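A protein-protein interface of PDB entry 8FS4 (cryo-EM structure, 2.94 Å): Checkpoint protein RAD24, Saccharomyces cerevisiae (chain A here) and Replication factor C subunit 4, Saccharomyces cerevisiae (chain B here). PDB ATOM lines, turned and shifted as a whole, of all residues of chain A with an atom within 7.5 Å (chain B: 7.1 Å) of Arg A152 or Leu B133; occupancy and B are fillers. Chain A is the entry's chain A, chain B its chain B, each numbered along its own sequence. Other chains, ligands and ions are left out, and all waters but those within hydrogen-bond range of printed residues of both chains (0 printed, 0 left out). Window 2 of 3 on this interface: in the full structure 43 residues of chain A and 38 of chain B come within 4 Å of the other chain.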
ATOM      1  N   GLU A  68     -18.442  18.146 -27.539  1.00  0.00           N
ATOM      2  CA  GLU A  68     -17.958  18.626 -28.826  1.00  0.00           C
ATOM      3  C   GLU A  68     -18.921  18.349 -29.969  1.00  0.00           C
ATOM      4  O   GLU A  68     -18.822  19.017 -31.007  1.00  0.00           O
ATOM      5  CB  GLU A  68     -16.610  17.980 -29.164  1.00  0.00           C
ATOM      6  CG  GLU A  68     -15.686  18.863 -29.990  1.00  0.00           C
ATOM      7  CD  GLU A  68     -14.954  18.099 -31.076  1.00  0.00           C
ATOM      8  OE1 GLU A  68     -15.231  16.899 -31.256  1.00  0.00           O
ATOM      9  OE2 GLU A  68     -14.077  18.696 -31.737  1.00  0.00           O
ATOM     10  N   THR A 149      -9.220  34.639 -34.357  1.00  0.00           N
ATOM     11  CA  THR A 149      -7.774  34.851 -34.274  1.00  0.00           C
ATOM     12  C   THR A 149      -7.277  34.562 -32.857  1.00  0.00           C
ATOM     13  O   THR A 149      -6.954  35.481 -32.101  1.00  0.00           O
ATOM     14  CB  THR A 149      -7.427  36.280 -34.734  1.00  0.00           C
ATOM     15  OG1 THR A 149      -7.389  36.307 -36.164  1.00  0.00           O
ATOM     16  CG2 THR A 149      -6.040  36.761 -34.245  1.00  0.00           C
ATOM     17  N   GLU A 150      -7.299  33.300 -32.443  1.00  0.00           N
ATOM     18  CA  GLU A 150      -6.891  32.939 -31.093  1.00  0.00           C
ATOM     19  C   GLU A 150      -5.377  32.763 -31.016  1.00  0.00           C
ATOM     20  O   GLU A 150      -4.754  32.217 -31.931  1.00  0.00           O
ATOM     21  CB  GLU A 150      -7.600  31.662 -30.640  1.00  0.00           C
ATOM     22  CG  GLU A 150      -7.375  31.324 -29.180  1.00  0.00           C
ATOM     23  CD  GLU A 150      -8.328  30.255 -28.684  1.00  0.00           C
ATOM     24  OE1 GLU A 150      -9.268  29.906 -29.428  1.00  0.00           O
ATOM     25  OE2 GLU A 150      -8.140  29.765 -27.551  1.00  0.00           O
ATOM     26  N   PHE A 151      -4.795  33.238 -29.915  1.00  0.00           N
ATOM     27  CA  PHE A 151      -3.359  33.137 -29.694  1.00  0.00           C
ATOM     28  C   PHE A 151      -2.954  31.693 -29.413  1.00  0.00           C
ATOM     29  O   PHE A 151      -3.765  30.869 -28.979  1.00  0.00           O
ATOM     30  CB  PHE A 151      -2.946  34.034 -28.524  1.00  0.00           C
ATOM     31  CG  PHE A 151      -1.497  33.914 -28.142  1.00  0.00           C
ATOM     32  CD1 PHE A 151      -0.498  34.237 -29.041  1.00  0.00           C
ATOM     33  CD2 PHE A 151      -1.137  33.480 -26.879  1.00  0.00           C
ATOM     34  CE1 PHE A 151       0.834  34.126 -28.690  1.00  0.00           C
ATOM     35  CE2 PHE A 151       0.190  33.367 -26.522  1.00  0.00           C
ATOM     36  CZ  PHE A 151       1.178  33.692 -27.428  1.00  0.00           C
ATOM     37  N   ARG A 152      -1.679  31.386 -29.670  1.00  0.00           N
ATOM     38  CA  ARG A 152      -1.108  30.060 -29.419  1.00  0.00           C
ATOM     39  C   ARG A 152       0.146  30.241 -28.569  1.00  0.00           C
ATOM     40  O   ARG A 152       1.242  30.447 -29.098  1.00  0.00           O
ATOM     41  CB  ARG A 152      -0.795  29.329 -30.724  1.00  0.00           C
ATOM     42  CG  ARG A 152      -1.566  29.827 -31.930  1.00  0.00           C
ATOM     43  CD  ARG A 152      -1.890  28.699 -32.890  1.00  0.00           C
ATOM     44  NE  ARG A 152      -2.956  27.847 -32.378  1.00  0.00           N
ATOM     45  CZ  ARG A 152      -4.245  28.157 -32.408  1.00  0.00           C
ATOM     46  NH1 ARG A 152      -4.670  29.300 -32.922  1.00  0.00           N
ATOM     47  NH2 ARG A 152      -5.130  27.301 -31.906  1.00  0.00           N
ATOM     48  N   GLY A 153      -0.013  30.162 -27.252  1.00  0.00           N
ATOM     49  CA  GLY A 153       1.115  30.254 -26.344  1.00  0.00           C
ATOM     50  C   GLY A 153       2.069  29.084 -26.480  1.00  0.00           C
ATOM     51  O   GLY A 153       3.274  29.226 -26.269  1.00  0.00           O
ATOM     52  N   SER A 165       7.472  35.814 -27.921  1.00  0.00           N
ATOM     53  CA  SER A 165       6.656  35.272 -29.002  1.00  0.00           C
ATOM     54  C   SER A 165       5.279  35.919 -29.018  1.00  0.00           C
ATOM     55  O   SER A 165       4.754  36.259 -30.085  1.00  0.00           O
ATOM     56  CB  SER A 165       6.535  33.756 -28.852  1.00  0.00           C
ATOM     57  OG  SER A 165       5.880  33.419 -27.642  1.00  0.00           O
ATOM     58  N   PHE A 166       4.679  36.098 -27.840  1.00  0.00           N
ATOM     59  CA  PHE A 166       3.415  36.818 -27.749  1.00  0.00           C
ATOM     60  C   PHE A 166       3.562  38.248 -28.247  1.00  0.00           C
ATOM     61  O   PHE A 166       2.605  38.824 -28.777  1.00  0.00           O
ATOM     62  CB  PHE A 166       2.919  36.792 -26.302  1.00  0.00           C
ATOM     63  CG  PHE A 166       1.584  37.451 -26.094  1.00  0.00           C
ATOM     64  CD1 PHE A 166       0.458  37.001 -26.761  1.00  0.00           C
ATOM     65  CD2 PHE A 166       1.452  38.499 -25.201  1.00  0.00           C
ATOM     66  CE1 PHE A 166      -0.771  37.600 -26.558  1.00  0.00           C
ATOM     67  CE2 PHE A 166       0.227  39.099 -24.993  1.00  0.00           C
ATOM     68  CZ  PHE A 166      -0.885  38.648 -25.671  1.00  0.00           C
ATOM     69  N   PHE A 169       3.295  37.989 -31.917  1.00  0.00           N
ATOM     70  CA  PHE A 169       1.890  37.738 -32.215  1.00  0.00           C
ATOM     71  C   PHE A 169       1.074  39.020 -32.117  1.00  0.00           C
ATOM     72  O   PHE A 169       0.301  39.351 -33.023  1.00  0.00           O
ATOM     73  CB  PHE A 169       1.340  36.679 -31.262  1.00  0.00           C
ATOM     74  CG  PHE A 169      -0.141  36.769 -31.051  1.00  0.00           C
ATOM     75  CD1 PHE A 169      -1.017  36.226 -31.974  1.00  0.00           C
ATOM     76  CD2 PHE A 169      -0.658  37.389 -29.927  1.00  0.00           C
ATOM     77  CE1 PHE A 169      -2.378  36.304 -31.783  1.00  0.00           C
ATOM     78  CE2 PHE A 169      -2.020  37.468 -29.732  1.00  0.00           C
ATOM     79  CZ  PHE A 169      -2.881  36.924 -30.663  1.00  0.00           C
ATOM     80  N   LEU A 185      -9.098  36.951 -29.440  1.00  0.00           N
ATOM     81  CA  LEU A 185      -9.394  36.305 -28.171  1.00  0.00           C
ATOM     82  C   LEU A 185      -8.120  35.645 -27.660  1.00  0.00           C
ATOM     83  O   LEU A 185      -7.470  34.899 -28.397  1.00  0.00           O
ATOM     84  CB  LEU A 185     -10.520  35.284 -28.362  1.00  0.00           C
ATOM     85  CG  LEU A 185     -11.299  34.736 -27.167  1.00  0.00           C
ATOM     86  CD1 LEU A 185     -12.452  33.882 -27.662  1.00  0.00           C
ATOM     87  CD2 LEU A 185     -10.419  33.935 -26.256  1.00  0.00           C
ATOM     88  N   ILE A 186      -7.770  35.913 -26.401  1.00  0.00           N
ATOM     89  CA  ILE A 186      -6.473  35.514 -25.859  1.00  0.00           C
ATOM     90  C   ILE A 186      -6.661  34.469 -24.769  1.00  0.00           C
ATOM     91  O   ILE A 186      -5.975  34.494 -23.742  1.00  0.00           O
ATOM     92  CB  ILE A 186      -5.676  36.719 -25.323  1.00  0.00           C
ATOM     93  CG1 ILE A 186      -5.761  37.898 -26.295  1.00  0.00           C
ATOM     94  CG2 ILE A 186      -4.214  36.328 -25.109  1.00  0.00           C
ATOM     95  CD1 ILE A 186      -4.796  39.029 -25.977  1.00  0.00           C
ATOM     96  N   ASP A 188      -5.557  31.733 -24.751  1.00  0.00           N
ATOM     97  CA  ASP A 188      -4.212  31.203 -24.555  1.00  0.00           C
ATOM     98  C   ASP A 188      -3.374  32.269 -23.863  1.00  0.00           C
ATOM     99  O   ASP A 188      -3.074  33.313 -24.451  1.00  0.00           O
ATOM    100  CB  ASP A 188      -3.591  30.800 -25.887  1.00  0.00           C
ATOM    101  CG  ASP A 188      -3.879  29.361 -26.248  1.00  0.00           C
ATOM    102  OD1 ASP A 188      -4.782  28.760 -25.629  1.00  0.00           O
ATOM    103  OD2 ASP A 188      -3.207  28.829 -27.154  1.00  0.00           O
ATOM    104  N   LEU A 189      -2.992  32.006 -22.617  1.00  0.00           N
ATOM    105  CA  LEU A 189      -2.243  32.973 -21.836  1.00  0.00           C
ATOM    106  C   LEU A 189      -0.761  32.650 -21.935  1.00  0.00           C
ATOM    107  O   LEU A 189      -0.345  31.574 -21.478  1.00  0.00           O
ATOM    108  CB  LEU A 189      -2.697  32.951 -20.376  1.00  0.00           C
ATOM    109  CG  LEU A 189      -4.086  33.531 -20.099  1.00  0.00           C
ATOM    110  CD1 LEU A 189      -4.431  33.407 -18.624  1.00  0.00           C
ATOM    111  CD2 LEU A 189      -4.179  34.982 -20.549  1.00  0.00           C
ATOM    112  N   PRO A 190       0.072  33.523 -22.526  1.00  0.00           N
ATOM    113  CA  PRO A 190       1.521  33.299 -22.465  1.00  0.00           C
ATOM    114  C   PRO A 190       1.932  32.958 -21.047  1.00  0.00           C
ATOM    115  O   PRO A 190       1.438  33.590 -20.113  1.00  0.00           O
ATOM    116  CB  PRO A 190       2.108  34.640 -22.917  1.00  0.00           C
ATOM    117  CG  PRO A 190       1.060  35.250 -23.756  1.00  0.00           C
ATOM    118  CD  PRO A 190      -0.266  34.757 -23.255  1.00  0.00           C
ATOM    119  N   LYS B  94       3.321  17.357 -27.946  1.00  0.00           N
ATOM    120  CA  LYS B  94       2.709  17.988 -29.107  1.00  0.00           C
ATOM    121  C   LYS B  94       3.026  17.237 -30.394  1.00  0.00           C
ATOM    122  O   LYS B  94       2.129  17.024 -31.219  1.00  0.00           O
ATOM    123  CB  LYS B  94       3.168  19.442 -29.224  1.00  0.00           C
ATOM    124  CG  LYS B  94       2.560  20.196 -30.397  1.00  0.00           C
ATOM    125  CD  LYS B  94       3.000  21.648 -30.400  1.00  0.00           C
ATOM    126  CE  LYS B  94       2.641  22.346 -31.703  1.00  0.00           C
ATOM    127  NZ  LYS B  94       3.380  21.790 -32.871  1.00  0.00           N
ATOM    128  N   ALA B  97       0.953  14.074 -30.457  1.00  0.00           N
ATOM    129  CA  ALA B  97      -0.439  14.309 -30.820  1.00  0.00           C
ATOM    130  C   ALA B  97      -0.579  14.611 -32.305  1.00  0.00           C
ATOM    131  O   ALA B  97      -1.525  14.145 -32.952  1.00  0.00           O
ATOM    132  CB  ALA B  97      -1.013  15.451 -29.985  1.00  0.00           C
ATOM    133  N   GLN B  98       0.348  15.388 -32.868  1.00  0.00           N
ATOM    134  CA  GLN B  98       0.260  15.724 -34.285  1.00  0.00           C
ATOM    135  C   GLN B  98       0.559  14.532 -35.185  1.00  0.00           C
ATOM    136  O   GLN B  98       0.266  14.587 -36.384  1.00  0.00           O
ATOM    137  CB  GLN B  98       1.215  16.870 -34.613  1.00  0.00           C
ATOM    138  CG  GLN B  98       0.552  18.232 -34.633  1.00  0.00           C
ATOM    139  CD  GLN B  98       1.551  19.359 -34.780  1.00  0.00           C
ATOM    140  OE1 GLN B  98       2.740  19.125 -34.984  1.00  0.00           O
ATOM    141  NE2 GLN B  98       1.069  20.592 -34.681  1.00  0.00           N
ATOM    142  N   LEU B 127      -0.945  21.615 -21.330  1.00  0.00           N
ATOM    143  CA  LEU B 127      -1.676  20.388 -21.599  1.00  0.00           C
ATOM    144  C   LEU B 127      -3.109  20.700 -21.980  1.00  0.00           C
ATOM    145  O   LEU B 127      -3.719  19.970 -22.762  1.00  0.00           O
ATOM    146  CB  LEU B 127      -1.646  19.472 -20.377  1.00  0.00           C
ATOM    147  CG  LEU B 127      -0.579  18.381 -20.296  1.00  0.00           C
ATOM    148  CD1 LEU B 127      -0.913  17.462 -19.141  1.00  0.00           C
ATOM    149  CD2 LEU B 127      -0.461  17.588 -21.584  1.00  0.00           C
ATOM    150  N   ARG B 128      -3.669  21.774 -21.427  1.00  0.00           N
ATOM    151  CA  ARG B 128      -5.005  22.181 -21.849  1.00  0.00           C
ATOM    152  C   ARG B 128      -5.027  22.521 -23.332  1.00  0.00           C
ATOM    153  O   ARG B 128      -5.949  22.126 -24.055  1.00  0.00           O
ATOM    154  CB  ARG B 128      -5.481  23.378 -21.038  1.00  0.00           C
ATOM    155  CG  ARG B 128      -5.691  23.100 -19.577  1.00  0.00           C
ATOM    156  CD  ARG B 128      -5.846  24.405 -18.844  1.00  0.00           C
ATOM    157  NE  ARG B 128      -6.955  25.176 -19.392  1.00  0.00           N
ATOM    158  CZ  ARG B 128      -7.321  26.374 -18.961  1.00  0.00           C
ATOM    159  NH1 ARG B 128      -6.694  26.971 -17.961  1.00  0.00           N
ATOM    160  NH2 ARG B 128      -8.344  26.988 -19.548  1.00  0.00           N
ATOM    161  N   ARG B 129      -4.019  23.255 -23.804  1.00  0.00           N
ATOM    162  CA  ARG B 129      -3.945  23.580 -25.223  1.00  0.00           C
ATOM    163  C   ARG B 129      -3.863  22.313 -26.061  1.00  0.00           C
ATOM    164  O   ARG B 129      -4.554  22.180 -27.080  1.00  0.00           O
ATOM    165  CB  ARG B 129      -2.737  24.491 -25.473  1.00  0.00           C
ATOM    166  CG  ARG B 129      -2.184  24.528 -26.903  1.00  0.00           C
ATOM    167  CD  ARG B 129      -2.864  25.593 -27.744  1.00  0.00           C
ATOM    168  NE  ARG B 129      -4.317  25.481 -27.713  1.00  0.00           N
ATOM    169  CZ  ARG B 129      -5.151  26.458 -28.040  1.00  0.00           C
ATOM    170  NH1 ARG B 129      -4.711  27.638 -28.444  1.00  0.00           N
ATOM    171  NH2 ARG B 129      -6.461  26.246 -27.967  1.00  0.00           N
ATOM    172  N   THR B 130      -3.020  21.368 -25.644  1.00  0.00           N
ATOM    173  CA  THR B 130      -2.888  20.134 -26.417  1.00  0.00           C
ATOM    174  C   THR B 130      -4.183  19.325 -26.397  1.00  0.00           C
ATOM    175  O   THR B 130      -4.595  18.781 -27.428  1.00  0.00           O
ATOM    176  CB  THR B 130      -1.722  19.296 -25.895  1.00  0.00           C
ATOM    177  OG1 THR B 130      -0.550  20.114 -25.797  1.00  0.00           O
ATOM    178  CG2 THR B 130      -1.436  18.132 -26.838  1.00  0.00           C
ATOM    179  N   MET B 131      -4.839  19.236 -25.239  1.00  0.00           N
ATOM    180  CA  MET B 131      -6.101  18.518 -25.113  1.00  0.00           C
ATOM    181  C   MET B 131      -7.232  19.183 -25.879  1.00  0.00           C
ATOM    182  O   MET B 131      -8.209  18.508 -26.215  1.00  0.00           O
ATOM    183  CB  MET B 131      -6.501  18.413 -23.641  1.00  0.00           C
ATOM    184  CG  MET B 131      -5.584  17.542 -22.791  1.00  0.00           C
ATOM    185  SD  MET B 131      -6.212  17.126 -21.147  1.00  0.00           S
ATOM    186  CE  MET B 131      -7.966  16.940 -21.435  1.00  0.00           C
ATOM    187  N   GLU B 132      -7.133  20.483 -26.139  1.00  0.00           N
ATOM    188  CA  GLU B 132      -8.155  21.202 -26.887  1.00  0.00           C
ATOM    189  C   GLU B 132      -7.939  21.117 -28.391  1.00  0.00           C
ATOM    190  O   GLU B 132      -8.905  20.944 -29.138  1.00  0.00           O
ATOM    191  CB  GLU B 132      -8.178  22.670 -26.438  1.00  0.00           C
ATOM    192  CG  GLU B 132      -8.501  23.703 -27.513  1.00  0.00           C
ATOM    193  CD  GLU B 132      -9.855  23.494 -28.168  1.00  0.00           C
ATOM    194  OE1 GLU B 132     -10.459  22.419 -27.986  1.00  0.00           O
ATOM    195  OE2 GLU B 132     -10.310  24.412 -28.886  1.00  0.00           O
ATOM    196  N   LEU B 133      -6.692  21.211 -28.857  1.00  0.00           N
ATOM    197  CA  LEU B 133      -6.460  21.232 -30.298  1.00  0.00           C
ATOM    198  C   LEU B 133      -6.425  19.834 -30.910  1.00  0.00           C
ATOM    199  O   LEU B 133      -6.731  19.683 -32.098  1.00  0.00           O
ATOM    200  CB  LEU B 133      -5.158  21.971 -30.605  1.00  0.00           C
ATOM    201  CG  LEU B 133      -5.163  22.796 -31.895  1.00  0.00           C
ATOM    202  CD1 LEU B 133      -5.837  24.139 -31.673  1.00  0.00           C
ATOM    203  CD2 LEU B 133      -3.749  22.995 -32.407  1.00  0.00           C
ATOM    204  N   TYR B 134      -6.070  18.810 -30.136  1.00  0.00           N
ATOM    205  CA  TYR B 134      -5.879  17.455 -30.646  1.00  0.00           C
ATOM    206  C   TYR B 134      -6.735  16.444 -29.893  1.00  0.00           C
ATOM    207  O   TYR B 134      -6.263  15.375 -29.505  1.00  0.00           O
ATOM    208  CB  TYR B 134      -4.411  17.045 -30.564  1.00  0.00           C
ATOM    209  CG  TYR B 134      -3.445  18.100 -31.038  1.00  0.00           C
ATOM    210  CD1 TYR B 134      -3.548  18.641 -32.309  1.00  0.00           C
ATOM    211  CD2 TYR B 134      -2.431  18.558 -30.211  1.00  0.00           C
ATOM    212  CE1 TYR B 134      -2.666  19.604 -32.745  1.00  0.00           C
ATOM    213  CE2 TYR B 134      -1.546  19.522 -30.636  1.00  0.00           C
ATOM    214  CZ  TYR B 134      -1.668  20.043 -31.903  1.00  0.00           C
ATOM    215  OH  TYR B 134      -0.785  21.007 -32.332  1.00  0.00           O
ATOM    216  N   SER B 135      -8.009  16.766 -29.675  1.00  0.00           N
ATOM    217  CA  SER B 135      -8.894  15.849 -28.969  1.00  0.00           C
ATOM    218  C   SER B 135      -9.441  14.746 -29.866  1.00  0.00           C
ATOM    219  O   SER B 135      -9.894  13.719 -29.352  1.00  0.00           O
ATOM    220  CB  SER B 135     -10.058  16.619 -28.346  1.00  0.00           C
ATOM    221  OG  SER B 135      -9.779  16.963 -27.000  1.00  0.00           O
ATOM    222  N   ASN B 136      -9.403  14.930 -31.186  1.00  0.00           N
ATOM    223  CA  ASN B 136     -10.015  13.988 -32.114  1.00  0.00           C
ATOM    224  C   ASN B 136      -9.099  12.834 -32.499  1.00  0.00           C
ATOM    225  O   ASN B 136      -9.573  11.872 -33.111  1.00  0.00           O
ATOM    226  CB  ASN B 136     -10.465  14.708 -33.394  1.00  0.00           C
ATOM    227  CG  ASN B 136      -9.454  15.729 -33.881  1.00  0.00           C
ATOM    228  OD1 ASN B 136      -8.416  15.375 -34.438  1.00  0.00           O
ATOM    229  ND2 ASN B 136      -9.756  17.006 -33.672  1.00  0.00           N
ATOM    230  N   SER B 137      -7.817  12.901 -32.159  1.00  0.00           N
ATOM    231  CA  SER B 137      -6.853  11.877 -32.541  1.00  0.00           C
ATOM    232  C   SER B 137      -6.237  11.158 -31.355  1.00  0.00           C
ATOM    233  O   SER B 137      -6.048   9.941 -31.409  1.00  0.00           O
ATOM    234  CB  SER B 137      -5.735  12.501 -33.387  1.00  0.00           C
ATOM    235  OG  SER B 137      -4.495  11.863 -33.137  1.00  0.00           O
ATOM    236  N   ARG B 157     -12.337  18.758 -18.720  1.00  0.00           N
ATOM    237  CA  ARG B 157     -12.352  18.032 -19.984  1.00  0.00           C
ATOM    238  C   ARG B 157     -12.279  16.523 -19.804  1.00  0.00           C
ATOM    239  O   ARG B 157     -12.359  15.797 -20.799  1.00  0.00           O
ATOM    240  CB  ARG B 157     -11.191  18.491 -20.871  1.00  0.00           C
ATOM    241  CG  ARG B 157     -10.838  19.962 -20.730  1.00  0.00           C
ATOM    242  CD  ARG B 157      -9.916  20.432 -21.842  1.00  0.00           C
ATOM    243  NE  ARG B 157     -10.188  21.811 -22.231  1.00  0.00           N
ATOM    244  CZ  ARG B 157     -10.940  22.175 -23.261  1.00  0.00           C
ATOM    245  NH1 ARG B 157     -11.526  21.283 -24.044  1.00  0.00           N
ATOM    246  NH2 ARG B 157     -11.113  23.470 -23.512  1.00  0.00           N
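The side-chain carboxylate (OE2) of Glu A150 lies within salt-bridge range of the guanidinium group (NH2) of Arg B129 (3.9 Å). The backbone carbonyl oxygen of Phe A151 is in hydrogen-bond range of the guanidinium group of Arg B129 (3.4 Å). The side-chain carboxylate (OD1) of Asp A188 lies within salt-bridge range of the guanidinium group (NH1) of Arg B129, at 3.0 Å.
O of Glu A150 lies within hydrogen-bond range of NH1 of Arg A152, at 3.1 Å. O of Leu A185 lies within hydrogen-bond range of N of Phe A151, at 3.5 Å. N of Gly A153 lies within hydrogen-bond range of OD2 of Asp A188 (3.5 Å).
Among the printed residues, merely in contact across the chains: Arg A152 with Arg B129 and Arg A152 with Leu B133.
Of the printed residues of chain B, Glu A150 touches Arg B129 (3.9 Å). Printed residues of chain B within 4 Å of Phe A151: Arg B129 (3.4 Å). Arg A152 touches two residues of chain B. Printed residues of chain B within 4 Å of Asp A188: Arg B129. Printed residues of chain A within 4 Å of Arg B129: Glu A150, Phe A151, Arg A152 and Asp A188. Of chain A, only Arg A152 comes within 4 Å of Leu B133. The nearest residue of chain B that does not touch Arg A152 is Glu B132 (6.6 Å). The nearest residue of chain A that does not touch Leu B133 is Asp A188 (7.0 Å). The nearest printed residue of chain B that does not touch Asp A188 is Glu B132 (6.6 Å).
Of the 14 printed residues of chain A, 4 touch a printed residue of chain B. Hydrophobic or aromatic side chains of chain B that line the printed part of chain A: Leu B133. Among the printed residues, Asp or Glu carboxylates within 4 Å of a Lys or Arg side-chain nitrogen of the other chain: Glu A150 with Arg B129 (3.9 Å) and Asp A188 with Arg B129 (2.3 Å).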
